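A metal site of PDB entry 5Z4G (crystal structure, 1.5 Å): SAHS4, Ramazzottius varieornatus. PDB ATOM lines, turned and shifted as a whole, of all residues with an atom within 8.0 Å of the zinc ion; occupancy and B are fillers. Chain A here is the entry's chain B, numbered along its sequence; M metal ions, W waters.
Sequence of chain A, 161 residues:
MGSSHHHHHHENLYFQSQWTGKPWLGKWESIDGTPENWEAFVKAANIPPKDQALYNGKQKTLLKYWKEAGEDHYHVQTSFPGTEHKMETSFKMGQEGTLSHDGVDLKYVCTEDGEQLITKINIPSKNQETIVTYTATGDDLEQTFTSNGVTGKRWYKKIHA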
ATOM      1  N   TRP A  66      -6.161  30.841  24.149  1.00  0.00           N
ATOM      2  CA  TRP A  66      -5.704  29.957  25.213  1.00  0.00           C
ATOM      3  C   TRP A  66      -5.305  28.574  24.743  1.00  0.00           C
ATOM      4  O   TRP A  66      -5.622  28.158  23.612  1.00  0.00           O
ATOM      5  CB  TRP A  66      -6.702  29.919  26.398  1.00  0.00           C
ATOM      6  CG  TRP A  66      -7.980  29.163  26.199  1.00  0.00           C
ATOM      7  CD1 TRP A  66      -8.271  27.913  26.679  1.00  0.00           C
ATOM      8  CD2 TRP A  66      -9.154  29.612  25.521  1.00  0.00           C
ATOM      9  NE1 TRP A  66      -9.553  27.556  26.328  1.00  0.00           N
ATOM     10  CE2 TRP A  66     -10.121  28.581  25.615  1.00  0.00           C
ATOM     11  CE3 TRP A  66      -9.486  30.787  24.818  1.00  0.00           C
ATOM     12  CZ2 TRP A  66     -11.398  28.688  25.050  1.00  0.00           C
ATOM     13  CZ3 TRP A  66     -10.747  30.890  24.238  1.00  0.00           C
ATOM     14  CH2 TRP A  66     -11.684  29.848  24.363  1.00  0.00           C
ATOM     15  N   LYS A  67      -4.583  27.883  25.633  1.00  0.00           N
ATOM     16  CA  LYS A  67      -4.025  26.561  25.397  1.00  0.00           C
ATOM     17  C   LYS A  67      -4.289  25.729  26.655  1.00  0.00           C
ATOM     18  O   LYS A  67      -3.871  26.108  27.761  1.00  0.00           O
ATOM     19  CB  LYS A  67      -2.510  26.703  25.112  1.00  0.00           C
ATOM     20  CG  LYS A  67      -1.629  25.471  25.353  1.00  0.00           C
ATOM     21  CD  LYS A  67      -1.257  24.763  24.066  1.00  0.00           C
ATOM     22  CE  LYS A  67      -2.194  23.615  23.758  1.00  0.00           C
ATOM     23  NZ  LYS A  67      -1.769  22.902  22.521  1.00  0.00           N
ATOM     24  N   GLU A  68      -4.994  24.621  26.489  1.00  0.00           N
ATOM     25  CA  GLU A  68      -5.212  23.666  27.584  1.00  0.00           C
ATOM     26  C   GLU A  68      -4.042  22.682  27.544  1.00  0.00           C
ATOM     27  O   GLU A  68      -3.705  22.174  26.477  1.00  0.00           O
ATOM     28  CB  GLU A  68      -6.562  22.946  27.429  1.00  0.00           C
ATOM     29  CG  GLU A  68      -7.760  23.853  27.161  1.00  0.00           C
ATOM     30  CD  GLU A  68      -8.457  24.387  28.416  1.00  0.00           C
ATOM     31  OE1 GLU A  68      -7.844  24.407  29.505  1.00  0.00           O
ATOM     32  OE2 GLU A  68      -9.630  24.800  28.288  1.00  0.00           O
ATOM     33  N   GLY A  70      -3.421  19.555  28.344  1.00  0.00           N
ATOM     34  CA  GLY A  70      -3.629  18.206  27.793  1.00  0.00           C
ATOM     35  C   GLY A  70      -4.024  18.096  26.332  1.00  0.00           C
ATOM     36  O   GLY A  70      -4.186  16.986  25.816  1.00  0.00           O
ATOM     37  N   GLU A  71      -4.173  19.235  25.653  1.00  0.00           N
ATOM     38  CA  GLU A  71      -4.648  19.279  24.263  1.00  0.00           C
ATOM     39  C   GLU A  71      -3.545  19.686  23.277  1.00  0.00           C
ATOM     40  O   GLU A  71      -2.562  20.315  23.659  1.00  0.00           O
ATOM     41  CB  GLU A  71      -5.841  20.226  24.123  1.00  0.00           C
ATOM     42  CG  GLU A  71      -7.028  19.883  25.026  1.00  0.00           C
ATOM     43  CD  GLU A  71      -8.263  20.708  24.696  1.00  0.00           C
ATOM     44  OE1 GLU A  71      -8.172  21.960  24.628  1.00  0.00           O
ATOM     45  OE2 GLU A  71      -9.333  20.104  24.486  1.00  0.00           O
ATOM     46  N   ASP A  72      -3.729  19.303  22.013  1.00  0.00           N
ATOM     47  CA  ASP A  72      -2.745  19.598  20.961  1.00  0.00           C
ATOM     48  C   ASP A  72      -3.198  20.755  20.063  1.00  0.00           C
ATOM     49  O   ASP A  72      -2.595  20.990  19.008  1.00  0.00           O
ATOM     50  CB  ASP A  72      -2.467  18.333  20.129  1.00  0.00           C
ATOM     51  CG  ASP A  72      -3.685  17.849  19.348  1.00  0.00           C
ATOM     52  OD1 ASP A  72      -4.843  18.144  19.745  1.00  0.00           O
ATOM     53  OD2 ASP A  72      -3.474  17.164  18.330  1.00  0.00           O
ATOM     54  N   HIS A  73      -4.241  21.460  20.476  1.00  0.00           N
ATOM     55  CA  HIS A  73      -4.774  22.584  19.726  1.00  0.00           C
ATOM     56  C   HIS A  73      -4.873  23.838  20.597  1.00  0.00           C
ATOM     57  O   HIS A  73      -4.850  23.743  21.832  1.00  0.00           O
ATOM     58  CB  HIS A  73      -6.153  22.236  19.117  1.00  0.00           C
ATOM     59  CG  HIS A  73      -7.195  21.862  20.130  1.00  0.00           C
ATOM     60  ND1 HIS A  73      -7.524  20.548  20.400  1.00  0.00           N
ATOM     61  CD2 HIS A  73      -7.996  22.623  20.913  1.00  0.00           C
ATOM     62  CE1 HIS A  73      -8.481  20.519  21.315  1.00  0.00           C
ATOM     63  NE2 HIS A  73      -8.781  21.769  21.643  1.00  0.00           N
ATOM     64  N   TYR A  74      -4.980  24.996  19.940  1.00  0.00           N
ATOM     65  CA  TYR A  74      -5.203  26.275  20.601  1.00  0.00           C
ATOM     66  C   TYR A  74      -6.643  26.678  20.426  1.00  0.00           C
ATOM     67  O   TYR A  74      -7.285  26.279  19.455  1.00  0.00           O
ATOM     68  CB  TYR A  74      -4.307  27.352  19.985  1.00  0.00           C
ATOM     69  CG  TYR A  74      -2.850  27.144  20.312  1.00  0.00           C
ATOM     70  CD1 TYR A  74      -2.044  26.302  19.524  1.00  0.00           C
ATOM     71  CD2 TYR A  74      -2.264  27.785  21.421  1.00  0.00           C
ATOM     72  CE1 TYR A  74      -0.710  26.089  19.850  1.00  0.00           C
ATOM     73  CE2 TYR A  74      -0.934  27.591  21.736  1.00  0.00           C
ATOM     74  CZ  TYR A  74      -0.162  26.751  20.948  1.00  0.00           C
ATOM     75  OH  TYR A  74       1.156  26.553  21.278  1.00  0.00           O
ATOM     76  N   HIS A  75      -7.137  27.480  21.357  1.00  0.00           N
ATOM     77  CA  HIS A  75      -8.478  28.034  21.270  1.00  0.00           C
ATOM     78  C   HIS A  75      -8.401  29.541  21.082  1.00  0.00           C
ATOM     79  O   HIS A  75      -7.511  30.202  21.619  1.00  0.00           O
ATOM     80  CB  HIS A  75      -9.260  27.741  22.546  1.00  0.00           C
ATOM     81  CG  HIS A  75      -9.811  26.360  22.635  1.00  0.00           C
ATOM     82  ND1 HIS A  75     -11.081  26.041  22.190  1.00  0.00           N
ATOM     83  CD2 HIS A  75      -9.290  25.216  23.130  1.00  0.00           C
ATOM     84  CE1 HIS A  75     -11.304  24.756  22.393  1.00  0.00           C
ATOM     85  NE2 HIS A  75     -10.235  24.232  22.961  1.00  0.00           N
ATOM     86  N   THR A  89     -13.353  29.190  17.991  1.00  0.00           N
ATOM     87  CA  THR A  89     -12.857  28.033  17.260  1.00  0.00           C
ATOM     88  C   THR A  89     -11.566  27.513  17.876  1.00  0.00           C
ATOM     89  O   THR A  89     -11.058  28.058  18.864  1.00  0.00           O
ATOM     90  CB  THR A  89     -12.710  28.321  15.731  1.00  0.00           C
ATOM     91  OG1 THR A  89     -12.642  27.086  14.995  1.00  0.00           O
ATOM     92  CG2 THR A  89     -11.492  29.200  15.400  1.00  0.00           C
ATOM     93  N   SER A  90     -11.056  26.431  17.302  1.00  0.00           N
ATOM     94  CA  SER A  90      -9.779  25.873  17.696  1.00  0.00           C
ATOM     95  C   SER A  90      -8.931  25.684  16.441  1.00  0.00           C
ATOM     96  O   SER A  90      -9.459  25.559  15.335  1.00  0.00           O
ATOM     97  CB  SER A  90      -9.966  24.546  18.435  1.00  0.00           C
ATOM     98  OG  SER A  90     -10.794  23.659  17.705  1.00  0.00           O
ATOM     99  N   PHE A  91      -7.619  25.682  16.628  1.00  0.00           N
ATOM    100  CA  PHE A  91      -6.692  25.510  15.512  1.00  0.00           C
ATOM    101  C   PHE A  91      -5.419  24.800  15.938  1.00  0.00           C
ATOM    102  O   PHE A  91      -5.053  24.815  17.124  1.00  0.00           O
ATOM    103  CB  PHE A  91      -6.368  26.874  14.833  1.00  0.00           C
ATOM    104  CG  PHE A  91      -5.674  27.862  15.719  1.00  0.00           C
ATOM    105  CD1 PHE A  91      -6.408  28.760  16.500  1.00  0.00           C
ATOM    106  CD2 PHE A  91      -4.274  27.925  15.773  1.00  0.00           C
ATOM    107  CE1 PHE A  91      -5.773  29.676  17.324  1.00  0.00           C
ATOM    108  CE2 PHE A  91      -3.628  28.834  16.591  1.00  0.00           C
ATOM    109  CZ  PHE A  91      -4.385  29.726  17.353  1.00  0.00           C
HETATM  110 ZN    ZN M   1      -9.977  22.253  23.332  1.00  0.00          ZN
HETATM  111  O   HOH W   1     -11.573  21.412  22.546  1.00  0.00           O
HETATM  112  O   HOH W   2     -11.020  22.428  25.341  1.00  0.00           O
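The backbone NH of His 75 is in hydrogen-bond range of the backbone carbonyl oxygen of Trp 66 (2.8 Å).
O of His 73 is in hydrogen-bond range of NZ of Lys 67, at 3.3 Å.
The backbone carbonyl oxygen (O) of Glu 71 sits at hydrogen-bond distance from the side-chain amino group (NZ) of Lys 67, at 2.9 Å.
Within 4 Å of the zinc ion: Glu 71, His 73 and His 75.
The nearest printed residue that does not touch the zinc ion is Glu 68 (4.7 Å).
The zinc ion is bound by water W1 (2.0 Å).
A ring nitrogen (NE2) of His 75 binds the zinc ion, at 2.0 Å.
The zinc ion is bound by NE2 of His 73.
The zinc ion is bound by the side-chain carboxylate (OE1) of Glu 71.
Water W2 is bound to the zinc ion (2.3 Å).
The zinc ion is bound by OE2 of Glu 71 (2.5 Å).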
